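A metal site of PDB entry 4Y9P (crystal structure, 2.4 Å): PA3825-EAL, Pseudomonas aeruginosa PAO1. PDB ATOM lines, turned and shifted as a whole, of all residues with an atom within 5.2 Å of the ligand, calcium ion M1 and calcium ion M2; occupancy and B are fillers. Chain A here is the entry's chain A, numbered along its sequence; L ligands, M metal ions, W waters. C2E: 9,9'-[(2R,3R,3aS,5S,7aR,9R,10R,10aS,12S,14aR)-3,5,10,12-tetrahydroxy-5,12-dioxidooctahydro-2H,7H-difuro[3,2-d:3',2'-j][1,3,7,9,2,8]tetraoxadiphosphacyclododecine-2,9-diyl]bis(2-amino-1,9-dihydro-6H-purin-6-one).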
ATOM      1  N   GLN A  25     -27.957 -18.661  -7.506  1.00  0.00           N
ATOM      2  CA  GLN A  25     -26.535 -18.369  -7.399  1.00  0.00           C
ATOM      3  C   GLN A  25     -26.155 -17.906  -5.957  1.00  0.00           C
ATOM      4  O   GLN A  25     -26.674 -16.853  -5.466  1.00  0.00           O
ATOM      5  CB  GLN A  25     -26.069 -17.288  -8.408  1.00  0.00           C
ATOM      6  CG  GLN A  25     -24.534 -17.160  -8.368  1.00  0.00           C
ATOM      7  CD  GLN A  25     -23.918 -16.305  -9.457  1.00  0.00           C
ATOM      8  OE1 GLN A  25     -24.470 -15.298  -9.796  1.00  0.00           O
ATOM      9  NE2 GLN A  25     -22.726 -16.664  -9.928  1.00  0.00           N
ATOM     10  N   GLU A  39     -29.170 -15.420  -5.227  1.00  0.00           N
ATOM     11  CA  GLU A  39     -29.933 -14.685  -6.262  1.00  0.00           C
ATOM     12  C   GLU A  39     -30.663 -15.712  -7.058  1.00  0.00           C
ATOM     13  O   GLU A  39     -30.062 -16.694  -7.477  1.00  0.00           O
ATOM     14  CB  GLU A  39     -29.026 -13.845  -7.208  1.00  0.00           C
ATOM     15  CG  GLU A  39     -29.829 -12.926  -8.133  1.00  0.00           C
ATOM     16  CD  GLU A  39     -29.009 -12.126  -9.162  1.00  0.00           C
ATOM     17  OE1 GLU A  39     -27.764 -12.198  -9.105  1.00  0.00           O
ATOM     18  OE2 GLU A  39     -29.656 -11.424 -10.033  1.00  0.00           O
ATOM     19  N   VAL A  40     -31.960 -15.513  -7.232  1.00  0.00           N
ATOM     20  CA  VAL A  40     -32.747 -16.424  -7.976  1.00  0.00           C
ATOM     21  C   VAL A  40     -32.673 -15.980  -9.401  1.00  0.00           C
ATOM     22  O   VAL A  40     -33.020 -14.805  -9.677  1.00  0.00           O
ATOM     23  CB  VAL A  40     -34.224 -16.351  -7.540  1.00  0.00           C
ATOM     24  CG1 VAL A  40     -35.086 -17.165  -8.483  1.00  0.00           C
ATOM     25  CG2 VAL A  40     -34.312 -16.809  -6.103  1.00  0.00           C
ATOM     26  N   LEU A  41     -32.214 -16.860 -10.283  1.00  0.00           N
ATOM     27  CA  LEU A  41     -32.117 -16.554 -11.732  1.00  0.00           C
ATOM     28  C   LEU A  41     -33.069 -17.426 -12.579  1.00  0.00           C
ATOM     29  O   LEU A  41     -33.124 -18.632 -12.409  1.00  0.00           O
ATOM     30  CB  LEU A  41     -30.677 -16.772 -12.210  1.00  0.00           C
ATOM     31  CG  LEU A  41     -29.521 -15.818 -11.940  1.00  0.00           C
ATOM     32  CD1 LEU A  41     -29.878 -14.653 -11.060  1.00  0.00           C
ATOM     33  CD2 LEU A  41     -28.372 -16.606 -11.349  1.00  0.00           C
ATOM     34  N   MET A  42     -33.822 -16.813 -13.465  1.00  0.00           N
ATOM     35  CA  MET A  42     -34.766 -17.563 -14.234  1.00  0.00           C
ATOM     36  C   MET A  42     -34.098 -18.410 -15.291  1.00  0.00           C
ATOM     37  O   MET A  42     -33.135 -18.022 -15.920  1.00  0.00           O
ATOM     38  CB  MET A  42     -35.783 -16.656 -14.893  1.00  0.00           C
ATOM     39  CG  MET A  42     -37.046 -17.402 -15.292  1.00  0.00           C
ATOM     40  SD  MET A  42     -38.356 -16.274 -15.912  1.00  0.00           S
ATOM     41  CE  MET A  42     -38.611 -15.136 -14.555  1.00  0.00           C
ATOM     42  N   ARG A  43     -34.638 -19.588 -15.481  1.00  0.00           N
ATOM     43  CA  ARG A  43     -34.225 -20.446 -16.555  1.00  0.00           C
ATOM     44  C   ARG A  43     -35.453 -20.964 -17.206  1.00  0.00           C
ATOM     45  O   ARG A  43     -36.472 -21.196 -16.540  1.00  0.00           O
ATOM     46  CB  ARG A  43     -33.361 -21.601 -16.009  1.00  0.00           C
ATOM     47  CG  ARG A  43     -31.984 -21.190 -15.481  1.00  0.00           C
ATOM     48  CD  ARG A  43     -31.030 -20.827 -16.606  1.00  0.00           C
ATOM     49  NE  ARG A  43     -29.697 -20.418 -16.134  1.00  0.00           N
ATOM     50  CZ  ARG A  43     -29.370 -19.191 -15.693  1.00  0.00           C
ATOM     51  NH1 ARG A  43     -30.257 -18.207 -15.661  1.00  0.00           N
ATOM     52  NH2 ARG A  43     -28.121 -18.930 -15.326  1.00  0.00           N
ATOM     53  N   ARG A  53     -31.471 -19.531 -21.747  1.00  0.00           N
ATOM     54  CA  ARG A  53     -31.067 -18.528 -20.776  1.00  0.00           C
ATOM     55  C   ARG A  53     -31.811 -17.209 -20.956  1.00  0.00           C
ATOM     56  O   ARG A  53     -32.275 -16.897 -22.064  1.00  0.00           O
ATOM     57  CB  ARG A  53     -29.603 -18.293 -20.863  1.00  0.00           C
ATOM     58  CG  ARG A  53     -28.809 -18.882 -19.718  1.00  0.00           C
ATOM     59  CD  ARG A  53     -27.396 -18.314 -19.831  1.00  0.00           C
ATOM     60  NE  ARG A  53     -26.772 -18.156 -18.538  1.00  0.00           N
ATOM     61  CZ  ARG A  53     -25.810 -17.295 -18.229  1.00  0.00           C
ATOM     62  NH1 ARG A  53     -25.287 -16.437 -19.108  1.00  0.00           N
ATOM     63  NH2 ARG A  53     -25.353 -17.286 -16.965  1.00  0.00           N
ATOM     64  N   PRO A  54     -31.930 -16.445 -19.876  1.00  0.00           N
ATOM     65  CA  PRO A  54     -32.785 -15.240 -19.776  1.00  0.00           C
ATOM     66  C   PRO A  54     -32.714 -14.211 -20.884  1.00  0.00           C
ATOM     67  O   PRO A  54     -33.751 -13.644 -21.273  1.00  0.00           O
ATOM     68  CB  PRO A  54     -32.351 -14.581 -18.461  1.00  0.00           C
ATOM     69  CG  PRO A  54     -31.749 -15.683 -17.639  1.00  0.00           C
ATOM     70  CD  PRO A  54     -31.203 -16.697 -18.594  1.00  0.00           C
ATOM     71  N   ASP A  55     -31.506 -13.930 -21.356  1.00  0.00           N
ATOM     72  CA  ASP A  55     -31.313 -12.859 -22.332  1.00  0.00           C
ATOM     73  C   ASP A  55     -31.972 -13.166 -23.642  1.00  0.00           C
ATOM     74  O   ASP A  55     -32.292 -12.255 -24.356  1.00  0.00           O
ATOM     75  CB  ASP A  55     -29.815 -12.501 -22.513  1.00  0.00           C
ATOM     76  CG  ASP A  55     -29.198 -11.833 -21.237  1.00  0.00           C
ATOM     77  OD1 ASP A  55     -29.931 -11.327 -20.343  1.00  0.00           O
ATOM     78  OD2 ASP A  55     -27.959 -11.820 -21.129  1.00  0.00           O
ATOM     79  N   ILE A  58     -36.265 -12.840 -21.548  1.00  0.00           N
ATOM     80  CA  ILE A  58     -36.720 -11.750 -20.666  1.00  0.00           C
ATOM     81  C   ILE A  58     -37.078 -10.470 -21.417  1.00  0.00           C
ATOM     82  O   ILE A  58     -38.083  -9.841 -21.102  1.00  0.00           O
ATOM     83  CB  ILE A  58     -35.710 -11.442 -19.537  1.00  0.00           C
ATOM     84  CG1 ILE A  58     -35.667 -12.578 -18.525  1.00  0.00           C
ATOM     85  CG2 ILE A  58     -36.052 -10.138 -18.827  1.00  0.00           C
ATOM     86  CD1 ILE A  58     -36.910 -12.735 -17.678  1.00  0.00           C
ATOM     87  N   GLU A  62     -40.847  -8.713 -20.973  1.00  0.00           N
ATOM     88  CA  GLU A  62     -41.009  -7.337 -20.491  1.00  0.00           C
ATOM     89  C   GLU A  62     -41.884  -6.522 -21.407  1.00  0.00           C
ATOM     90  O   GLU A  62     -42.784  -5.869 -20.934  1.00  0.00           O
ATOM     91  CB  GLU A  62     -39.644  -6.664 -20.231  1.00  0.00           C
ATOM     92  CG  GLU A  62     -38.929  -7.307 -19.037  1.00  0.00           C
ATOM     93  CD  GLU A  62     -37.574  -6.712 -18.689  1.00  0.00           C
ATOM     94  OE1 GLU A  62     -36.871  -6.181 -19.580  1.00  0.00           O
ATOM     95  OE2 GLU A  62     -37.173  -6.827 -17.491  1.00  0.00           O
ATOM     96  N   ILE A  67     -43.751 -10.806 -18.025  1.00  0.00           N
ATOM     97  CA  ILE A  67     -42.705 -10.911 -16.994  1.00  0.00           C
ATOM     98  C   ILE A  67     -43.253 -10.813 -15.569  1.00  0.00           C
ATOM     99  O   ILE A  67     -42.756 -11.473 -14.636  1.00  0.00           O
ATOM    100  CB  ILE A  67     -41.577  -9.875 -17.223  1.00  0.00           C
ATOM    101  CG1 ILE A  67     -40.386 -10.130 -16.284  1.00  0.00           C
ATOM    102  CG2 ILE A  67     -42.079  -8.452 -17.051  1.00  0.00           C
ATOM    103  CD1 ILE A  67     -39.764 -11.509 -16.424  1.00  0.00           C
ATOM    104  N   THR A  71     -42.651 -13.785 -12.927  1.00  0.00           N
ATOM    105  CA  THR A  71     -41.923 -13.555 -11.704  1.00  0.00           C
ATOM    106  C   THR A  71     -42.715 -14.073 -10.494  1.00  0.00           C
ATOM    107  O   THR A  71     -42.152 -14.604  -9.503  1.00  0.00           O
ATOM    108  CB  THR A  71     -41.648 -12.055 -11.614  1.00  0.00           C
ATOM    109  OG1 THR A  71     -40.913 -11.668 -12.774  1.00  0.00           O
ATOM    110  CG2 THR A  71     -40.910 -11.694 -10.354  1.00  0.00           C
ATOM    111  N   LEU A  74     -42.288 -17.734 -10.235  1.00  0.00           N
ATOM    112  CA  LEU A  74     -40.917 -18.022  -9.774  1.00  0.00           C
ATOM    113  C   LEU A  74     -40.831 -17.883  -8.257  1.00  0.00           C
ATOM    114  O   LEU A  74     -40.334 -18.763  -7.591  1.00  0.00           O
ATOM    115  CB  LEU A  74     -39.930 -17.071 -10.459  1.00  0.00           C
ATOM    116  CG  LEU A  74     -38.491 -17.562 -10.507  1.00  0.00           C
ATOM    117  CD1 LEU A  74     -38.350 -18.660 -11.564  1.00  0.00           C
ATOM    118  CD2 LEU A  74     -37.585 -16.372 -10.825  1.00  0.00           C
ATOM    119  N   ASN A  98     -34.845 -10.695  -9.388  1.00  0.00           N
ATOM    120  CA  ASN A  98     -34.722  -9.607 -10.323  1.00  0.00           C
ATOM    121  C   ASN A  98     -36.134  -9.134 -10.673  1.00  0.00           C
ATOM    122  O   ASN A  98     -36.973  -9.941 -10.953  1.00  0.00           O
ATOM    123  CB  ASN A  98     -33.979 -10.090 -11.579  1.00  0.00           C
ATOM    124  CG  ASN A  98     -32.558 -10.434 -11.267  1.00  0.00           C
ATOM    125  OD1 ASN A  98     -31.735  -9.540 -11.117  1.00  0.00           O
ATOM    126  ND2 ASN A  98     -32.257 -11.725 -11.127  1.00  0.00           N
ATOM    127  N   ILE A  99     -36.376  -7.829 -10.670  1.00  0.00           N
ATOM    128  CA  ILE A  99     -37.719  -7.207 -10.826  1.00  0.00           C
ATOM    129  C   ILE A  99     -37.663  -6.279 -12.019  1.00  0.00           C
ATOM    130  O   ILE A  99     -36.698  -5.563 -12.185  1.00  0.00           O
ATOM    131  CB  ILE A  99     -37.995  -6.370  -9.529  1.00  0.00           C
ATOM    132  CG1 ILE A  99     -38.345  -7.261  -8.314  1.00  0.00           C
ATOM    133  CG2 ILE A  99     -39.085  -5.337  -9.644  1.00  0.00           C
ATOM    134  CD1 ILE A  99     -39.161  -8.488  -8.593  1.00  0.00           C
ATOM    135  N   SER A 100     -38.701  -6.267 -12.850  1.00  0.00           N
ATOM    136  CA  SER A 100     -38.780  -5.346 -13.977  1.00  0.00           C
ATOM    137  C   SER A 100     -39.401  -3.994 -13.609  1.00  0.00           C
ATOM    138  O   SER A 100     -40.028  -3.840 -12.580  1.00  0.00           O
ATOM    139  CB  SER A 100     -39.536  -5.948 -15.175  1.00  0.00           C
ATOM    140  OG  SER A 100     -40.511  -6.832 -14.716  1.00  0.00           O
ATOM    141  N   GLU A 130     -34.122  -6.676  -6.837  1.00  0.00           N
ATOM    142  CA  GLU A 130     -33.052  -6.069  -7.595  1.00  0.00           C
ATOM    143  C   GLU A 130     -33.663  -5.369  -8.771  1.00  0.00           C
ATOM    144  O   GLU A 130     -34.409  -5.952  -9.561  1.00  0.00           O
ATOM    145  CB  GLU A 130     -32.002  -7.102  -8.041  1.00  0.00           C
ATOM    146  CG  GLU A 130     -31.604  -8.110  -6.991  1.00  0.00           C
ATOM    147  CD  GLU A 130     -30.412  -8.974  -7.402  1.00  0.00           C
ATOM    148  OE1 GLU A 130     -29.986  -8.926  -8.588  1.00  0.00           O
ATOM    149  OE2 GLU A 130     -29.864  -9.686  -6.506  1.00  0.00           O
ATOM    150  N   ASP A 160     -29.217  -3.204  -9.173  1.00  0.00           N
ATOM    151  CA  ASP A 160     -28.495  -4.209  -9.935  1.00  0.00           C
ATOM    152  C   ASP A 160     -27.605  -3.499 -10.889  1.00  0.00           C
ATOM    153  O   ASP A 160     -27.903  -2.374 -11.263  1.00  0.00           O
ATOM    154  CB  ASP A 160     -29.461  -5.049 -10.734  1.00  0.00           C
ATOM    155  CG  ASP A 160     -29.002  -6.451 -10.925  1.00  0.00           C
ATOM    156  OD1 ASP A 160     -27.797  -6.735 -10.879  1.00  0.00           O
ATOM    157  OD2 ASP A 160     -29.891  -7.284 -11.103  1.00  0.00           O
ATOM    158  N   ASP A 161     -26.518  -4.145 -11.266  1.00  0.00           N
ATOM    159  CA  ASP A 161     -25.629  -3.622 -12.348  1.00  0.00           C
ATOM    160  C   ASP A 161     -25.279  -2.145 -12.176  1.00  0.00           C
ATOM    161  O   ASP A 161     -25.369  -1.359 -13.112  1.00  0.00           O
ATOM    162  CB  ASP A 161     -26.256  -3.898 -13.735  1.00  0.00           C
ATOM    163  CG  ASP A 161     -26.536  -5.410 -13.972  1.00  0.00           C
ATOM    164  OD1 ASP A 161     -25.845  -6.363 -13.414  1.00  0.00           O
ATOM    165  OD2 ASP A 161     -27.495  -5.601 -14.754  1.00  0.00           O
ATOM    166  N   LYS A 181     -25.450  -3.484  -6.010  1.00  0.00           N
ATOM    167  CA  LYS A 181     -24.672  -4.551  -6.662  1.00  0.00           C
ATOM    168  C   LYS A 181     -23.771  -4.028  -7.766  1.00  0.00           C
ATOM    169  O   LYS A 181     -24.200  -3.504  -8.796  1.00  0.00           O
ATOM    170  CB  LYS A 181     -25.604  -5.591  -7.213  1.00  0.00           C
ATOM    171  CG  LYS A 181     -26.556  -6.063  -6.147  1.00  0.00           C
ATOM    172  CD  LYS A 181     -27.345  -7.275  -6.587  1.00  0.00           C
ATOM    173  CE  LYS A 181     -26.564  -8.546  -6.526  1.00  0.00           C
ATOM    174  NZ  LYS A 181     -27.220  -9.597  -7.314  1.00  0.00           N
ATOM    175  N   ASP A 183     -21.854  -4.024 -10.851  1.00  0.00           N
ATOM    176  CA  ASP A 183     -21.791  -4.811 -12.101  1.00  0.00           C
ATOM    177  C   ASP A 183     -20.459  -5.563 -12.321  1.00  0.00           C
ATOM    178  O   ASP A 183     -19.344  -5.039 -12.052  1.00  0.00           O
ATOM    179  CB  ASP A 183     -21.989  -3.899 -13.288  1.00  0.00           C
ATOM    180  CG  ASP A 183     -22.269  -4.669 -14.565  1.00  0.00           C
ATOM    181  OD1 ASP A 183     -23.332  -5.334 -14.629  1.00  0.00           O
ATOM    182  OD2 ASP A 183     -21.421  -4.563 -15.472  1.00  0.00           O
ATOM    183  N   GLN A 184     -20.568  -6.721 -12.919  1.00  0.00           N
ATOM    184  CA  GLN A 184     -19.385  -7.529 -13.275  1.00  0.00           C
ATOM    185  C   GLN A 184     -18.370  -6.868 -14.170  1.00  0.00           C
ATOM    186  O   GLN A 184     -17.191  -7.230 -14.151  1.00  0.00           O
ATOM    187  CB  GLN A 184     -19.792  -8.917 -13.823  1.00  0.00           C
ATOM    188  CG  GLN A 184     -21.096  -9.024 -14.635  1.00  0.00           C
ATOM    189  CD  GLN A 184     -21.661 -10.438 -14.758  1.00  0.00           C
ATOM    190  OE1 GLN A 184     -21.426 -11.099 -15.767  1.00  0.00           O
ATOM    191  NE2 GLN A 184     -22.417 -10.928 -13.728  1.00  0.00           N
ATOM    192  N   GLU A 217     -20.513  -8.501  -7.992  1.00  0.00           N
ATOM    193  CA  GLU A 217     -20.936  -9.559  -8.946  1.00  0.00           C
ATOM    194  C   GLU A 217     -19.821  -9.913  -9.900  1.00  0.00           C
ATOM    195  O   GLU A 217     -19.021  -9.097 -10.220  1.00  0.00           O
ATOM    196  CB  GLU A 217     -22.060  -9.059  -9.846  1.00  0.00           C
ATOM    197  CG  GLU A 217     -23.374  -8.681  -9.181  1.00  0.00           C
ATOM    198  CD  GLU A 217     -24.359  -8.178 -10.289  1.00  0.00           C
ATOM    199  OE1 GLU A 217     -24.662  -8.910 -11.273  1.00  0.00           O
ATOM    200  OE2 GLU A 217     -24.783  -6.989 -10.267  1.00  0.00           O
ATOM    201  N   GLY A 218     -19.754 -11.164 -10.313  1.00  0.00           N
ATOM    202  CA  GLY A 218     -18.779 -11.634 -11.267  1.00  0.00           C
ATOM    203  C   GLY A 218     -17.392 -11.808 -10.710  1.00  0.00           C
ATOM    204  O   GLY A 218     -16.406 -11.708 -11.445  1.00  0.00           O
ATOM    205  N   VAL A 219     -17.277 -12.147  -9.434  1.00  0.00           N
ATOM    206  CA  VAL A 219     -15.952 -12.475  -8.873  1.00  0.00           C
ATOM    207  C   VAL A 219     -15.543 -13.872  -9.378  1.00  0.00           C
ATOM    208  O   VAL A 219     -16.214 -14.841  -9.112  1.00  0.00           O
ATOM    209  CB  VAL A 219     -16.016 -12.501  -7.347  1.00  0.00           C
ATOM    210  CG1 VAL A 219     -14.662 -12.800  -6.733  1.00  0.00           C
ATOM    211  CG2 VAL A 219     -16.535 -11.201  -6.854  1.00  0.00           C
ATOM    212  N   GLU A 220     -14.526 -13.925 -10.169  1.00  0.00           N
ATOM    213  CA  GLU A 220     -14.003 -15.163 -10.744  1.00  0.00           C
ATOM    214  C   GLU A 220     -12.597 -15.526 -10.269  1.00  0.00           C
ATOM    215  O   GLU A 220     -12.208 -16.680 -10.328  1.00  0.00           O
ATOM    216  CB  GLU A 220     -13.944 -15.022 -12.296  1.00  0.00           C
ATOM    217  CG  GLU A 220     -15.290 -14.704 -12.879  1.00  0.00           C
ATOM    218  CD  GLU A 220     -15.266 -14.441 -14.371  1.00  0.00           C
ATOM    219  OE1 GLU A 220     -14.193 -14.203 -14.990  1.00  0.00           O
ATOM    220  OE2 GLU A 220     -16.377 -14.408 -14.945  1.00  0.00           O
ATOM    221  N   GLN A 237     -20.262 -12.497  -5.263  1.00  0.00           N
ATOM    222  CA  GLN A 237     -21.079 -13.356  -6.088  1.00  0.00           C
ATOM    223  C   GLN A 237     -20.292 -13.560  -7.364  1.00  0.00           C
ATOM    224  O   GLN A 237     -19.630 -12.637  -7.886  1.00  0.00           O
ATOM    225  CB  GLN A 237     -22.426 -12.662  -6.269  1.00  0.00           C
ATOM    226  CG  GLN A 237     -23.355 -13.330  -7.180  1.00  0.00           C
ATOM    227  CD  GLN A 237     -24.708 -12.613  -7.295  1.00  0.00           C
ATOM    228  OE1 GLN A 237     -24.994 -11.581  -6.641  1.00  0.00           O
ATOM    229  NE2 GLN A 237     -25.590 -13.209  -8.107  1.00  0.00           N
ATOM    230  N   GLY A 238     -20.301 -14.784  -7.846  1.00  0.00           N
ATOM    231  CA  GLY A 238     -19.558 -15.060  -9.085  1.00  0.00           C
ATOM    232  C   GLY A 238     -19.167 -16.528  -9.145  1.00  0.00           C
ATOM    233  O   GLY A 238     -19.367 -17.250  -8.166  1.00  0.00           O
ATOM    234  N   TYR A 239     -18.538 -16.939 -10.278  1.00  0.00           N
ATOM    235  CA  TYR A 239     -18.047 -18.286 -10.471  1.00  0.00           C
ATOM    236  C   TYR A 239     -17.050 -18.692  -9.427  1.00  0.00           C
ATOM    237  O   TYR A 239     -16.997 -19.853  -9.166  1.00  0.00           O
ATOM    238  CB  TYR A 239     -17.473 -18.513 -11.885  1.00  0.00           C
ATOM    239  CG  TYR A 239     -18.548 -18.334 -12.997  1.00  0.00           C
ATOM    240  CD1 TYR A 239     -19.916 -18.476 -12.724  1.00  0.00           C
ATOM    241  CD2 TYR A 239     -18.216 -17.955 -14.264  1.00  0.00           C
ATOM    242  CE1 TYR A 239     -20.864 -18.331 -13.693  1.00  0.00           C
ATOM    243  CE2 TYR A 239     -19.184 -17.806 -15.244  1.00  0.00           C
ATOM    244  CZ  TYR A 239     -20.518 -18.019 -14.943  1.00  0.00           C
ATOM    245  OH  TYR A 239     -21.575 -17.866 -15.841  1.00  0.00           O
ATOM    246  N   LEU A 240     -16.324 -17.746  -8.814  1.00  0.00           N
ATOM    247  CA  LEU A 240     -15.413 -18.087  -7.733  1.00  0.00           C
ATOM    248  C   LEU A 240     -16.155 -18.711  -6.557  1.00  0.00           C
ATOM    249  O   LEU A 240     -15.692 -19.648  -6.002  1.00  0.00           O
ATOM    250  CB  LEU A 240     -14.590 -16.886  -7.256  1.00  0.00           C
ATOM    251  CG  LEU A 240     -13.388 -17.280  -6.320  1.00  0.00           C
ATOM    252  CD1 LEU A 240     -12.058 -17.305  -7.011  1.00  0.00           C
ATOM    253  CD2 LEU A 240     -13.197 -16.341  -5.170  1.00  0.00           C
ATOM    254  N   PRO A 244     -24.688 -20.337 -10.937  1.00  0.00           N
ATOM    255  CA  PRO A 244     -26.125 -20.520 -10.799  1.00  0.00           C
ATOM    256  C   PRO A 244     -26.409 -21.988 -10.871  1.00  0.00           C
ATOM    257  O   PRO A 244     -25.773 -22.642 -11.645  1.00  0.00           O
ATOM    258  CB  PRO A 244     -26.695 -19.838 -12.018  1.00  0.00           C
ATOM    259  CG  PRO A 244     -25.675 -18.858 -12.439  1.00  0.00           C
ATOM    260  CD  PRO A 244     -24.346 -19.412 -12.022  1.00  0.00           C
HETATM  261  P1  C2E L   1     -27.931  -9.997 -13.688  1.00  0.00           P
HETATM  262  O2P C2E L   1     -29.094 -10.195 -12.774  1.00  0.00           O
HETATM  263  O1P C2E L   1     -27.232  -8.653 -13.664  1.00  0.00           O
HETATM  264  O5' C2E L   1     -26.654 -10.897 -13.468  1.00  0.00           O
HETATM  265  C5' C2E L   1     -26.665 -12.272 -13.287  1.00  0.00           C
HETATM  266  C4' C2E L   1     -25.998 -12.823 -14.532  1.00  0.00           C
HETATM  267  O4' C2E L   1     -24.572 -12.976 -14.484  1.00  0.00           O
HETATM  268  C3' C2E L   1     -26.524 -14.210 -14.699  1.00  0.00           C
HETATM  269  O3' C2E L   1     -26.717 -14.488 -16.077  1.00  0.00           O
HETATM  270  C2' C2E L   1     -25.447 -15.041 -14.114  1.00  0.00           C
HETATM  271  O2' C2E L   1     -25.579 -16.357 -14.575  1.00  0.00           O
HETATM  272  C1' C2E L   1     -24.224 -14.348 -14.642  1.00  0.00           C
HETATM  273  N9  C2E L   1     -23.012 -14.585 -13.859  1.00  0.00           N
HETATM  274  C8  C2E L   1     -22.936 -14.894 -12.567  1.00  0.00           C
HETATM  275  N7  C2E L   1     -21.670 -14.971 -12.122  1.00  0.00           N
HETATM  276  C5  C2E L   1     -20.907 -14.727 -13.146  1.00  0.00           C
HETATM  277  C6  C2E L   1     -19.471 -14.670 -13.330  1.00  0.00           C
HETATM  278  O6  C2E L   1     -18.711 -14.892 -12.365  1.00  0.00           O
HETATM  279  N1  C2E L   1     -19.050 -14.364 -14.549  1.00  0.00           N
HETATM  280  C2  C2E L   1     -19.892 -14.114 -15.591  1.00  0.00           C
HETATM  281  N2  C2E L   1     -19.358 -13.823 -16.795  1.00  0.00           N
HETATM  282  N3  C2E L   1     -21.247 -14.149 -15.483  1.00  0.00           N
HETATM  283  C4  C2E L   1     -21.785 -14.468 -14.301  1.00  0.00           C
HETATM  284  P11 C2E L   1     -28.143 -15.091 -16.496  1.00  0.00           P
HETATM  285  O21 C2E L   1     -28.656 -16.093 -15.466  1.00  0.00           O
HETATM  286  O11 C2E L   1     -28.084 -15.391 -17.966  1.00  0.00           O
HETATM  287  O5A C2E L   1     -29.038 -13.764 -16.308  1.00  0.00           O
HETATM  288  C5A C2E L   1     -28.673 -12.608 -17.104  1.00  0.00           C
HETATM  289  C4A C2E L   1     -29.624 -11.473 -16.815  1.00  0.00           C
HETATM  290  O4A C2E L   1     -30.963 -11.885 -17.031  1.00  0.00           O
HETATM  291  C3A C2E L   1     -29.589 -11.081 -15.370  1.00  0.00           C
HETATM  292  O3A C2E L   1     -28.429 -10.307 -15.171  1.00  0.00           O
HETATM  293  C2A C2E L   1     -30.929 -10.412 -15.241  1.00  0.00           C
HETATM  294  O2A C2E L   1     -30.909  -9.136 -15.816  1.00  0.00           O
HETATM  295  C1A C2E L   1     -31.852 -11.200 -16.138  1.00  0.00           C
HETATM  296  N91 C2E L   1     -32.736 -12.087 -15.347  1.00  0.00           N
HETATM  297  C81 C2E L   1     -32.528 -13.352 -14.922  1.00  0.00           C
HETATM  298  N71 C2E L   1     -33.608 -13.827 -14.250  1.00  0.00           N
HETATM  299  C51 C2E L   1     -34.506 -12.826 -14.247  1.00  0.00           C
HETATM  300  C61 C2E L   1     -35.851 -12.623 -13.741  1.00  0.00           C
HETATM  301  O61 C2E L   1     -36.351 -13.575 -13.090  1.00  0.00           O
HETATM  302  N11 C2E L   1     -36.472 -11.437 -13.984  1.00  0.00           N
HETATM  303  C21 C2E L   1     -35.891 -10.434 -14.662  1.00  0.00           C
HETATM  304  N21 C2E L   1     -36.512  -9.247 -14.868  1.00  0.00           N
HETATM  305  N31 C2E L   1     -34.650 -10.573 -15.155  1.00  0.00           N
HETATM  306  C41 C2E L   1     -33.939 -11.700 -14.970  1.00  0.00           C
HETATM  307 CA    CA M   1     -29.408  -9.385 -10.778  1.00  0.00          CA
HETATM  308 CA    CA M   2     -24.354  -7.961 -13.417  1.00  0.00          CA
HETATM  309 CA    CA M   3     -34.134  -6.570 -13.881  1.00  0.00          CA
HETATM  310  O   HOH W   1     -27.238  -9.709 -10.070  1.00  0.00           O
HETATM  311  O   HOH W   2     -35.143 -13.245 -10.197  1.00  0.00           O
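The backbone NH (N) of Met 42 is in hydrogen-bond range of a nitrogen (N71) of the ligand (3.1 Å).
NE of Arg 53 is in salt-bridge range of O11 of the ligand, 3.1 Å away.
O1P of the ligand sits close to OD1 of Asp 161 (2.7 Å).
The side-chain carboxylate of Glu 220 is in hydrogen-bond range of a nitrogen (N1) of the ligand, at 2.7 Å.
NE2 of Gln 184 lies within hydrogen-bond range of O4' of the ligand, at 3.1 Å.
The guanidinium group (NH1) of Arg 43 lies within salt-bridge range of an oxygen (O21) of the ligand, at 2.7 Å.
NE2 of Gln 25 sits at hydrogen-bond distance from N7 of the ligand, at 3.0 Å.
An oxygen (O6) of the ligand is in hydrogen-bond range of the backbone NH (N) of Tyr 239.
O of Asn 98 sits at hydrogen-bond distance from N11 of the ligand.
NZ of Lys 181 lies within salt-bridge range of OE2 of Glu 130 (2.8 Å).
The backbone carbonyl oxygen (O) of Glu 130 is in hydrogen-bond range of the backbone NH (N) of Ile 99, 2.9 Å away.
The side-chain carboxylate (OE1) of Glu 39 is in salt-bridge range of the side-chain amino group (NZ) of Lys 181 (3.2 Å).
The backbone NH of Gly 218 is in hydrogen-bond range of the backbone carbonyl oxygen of Gln 237.
OE1 of Gln 25 sits at hydrogen-bond distance from NE2 of Gln 237 (2.9 Å).
N of Tyr 239 is in hydrogen-bond range of O of Val 219, at 3.3 Å.
NE2 of Gln 237 is in hydrogen-bond range of OE1 of Glu 39, 2.6 Å away.
The backbone carbonyl oxygen (O) of Glu 39 is in hydrogen-bond range of the backbone NH (N) of Gln 25 (2.9 Å).
Leu 41 touches the ligand (CG to O21, 3.6 Å).
Pro 54 touches the ligand.
Asp 55 touches the ligand (OD1 to O4A, 3.5 Å).
Ile 58 touches the ligand.
Glu 62 touches the ligand.
Leu 74 touches the ligand (CD2 to O61, 3.8 Å).
Gly 218 touches the ligand (CA to O6, 3.4 Å).
CA of Gly 238 touches O6 of the ligand, at 3.4 Å.
CG of Pro 244 touches O2' of the ligand, at 3.3 Å.
Hydrophobic or aromatic side chains that line the ligand: Leu 41, Met 42, Pro 54, Ile 58, Leu 74, Tyr 239 and Pro 244.
21 residues have an atom within 4 Å of the ligand: Gln 25, Glu 39, Leu 41, Met 42, Arg 43, Arg 53, Pro 54, Asp 55, Ile 58, Glu 62, Leu 74, Asn 98, Asp 160, Asp 161, Gln 184, Glu 217, Gly 218, Glu 220, Gly 238, Tyr 239 and Pro 244.
The nearest printed residue that does not touch the ligand is Ile 67 (4.1 Å).
Four residues have an atom within 4 Å of calcium ion M1: Glu 39, Asn 98, Glu 130 and Asp 160.
NE2 of Gln 184 touches calcium ion M2 (3.6 Å).
The nearest printed residue that does not touch calcium ion M2 is Asp 160 (4.4 Å).
Calcium ion M1 is bound by O2P of the ligand (2.2 Å), OD2 of Asp 160 (2.2 Å), OE2 of Glu 39 (2.2 Å), water W1 (2.3 Å), OE1 of Glu 130 (2.3 Å) and OD1 of Asn 98 (2.4 Å).
Slightly farther from calcium ion M1 lies the side-chain carboxylate (OD1) of Asp 160 (3.1 Å).
OD1 of Asp 161 is bound to calcium ion M2.
OE1 of Glu 217 binds calcium ion M2, 2.4 Å away.
Slightly farther from calcium ion M2 lies O1P of the ligand (3.0 Å).
Slightly farther from calcium ion M2 lies OD1 of Asp 183 (3.1 Å).
Water W1 lies within hydrogen-bond range of the side-chain carboxylate of Glu 39 (2.7 Å), the side-chain amino group of Lys 181 (2.8 Å) and the side-chain carboxylate of Asp 160 (3.1 Å).
Water W2 lies within hydrogen-bond range of the backbone carbonyl oxygen of Val 40, the backbone NH of Asn 98 and an oxygen (O61) of the ligand.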
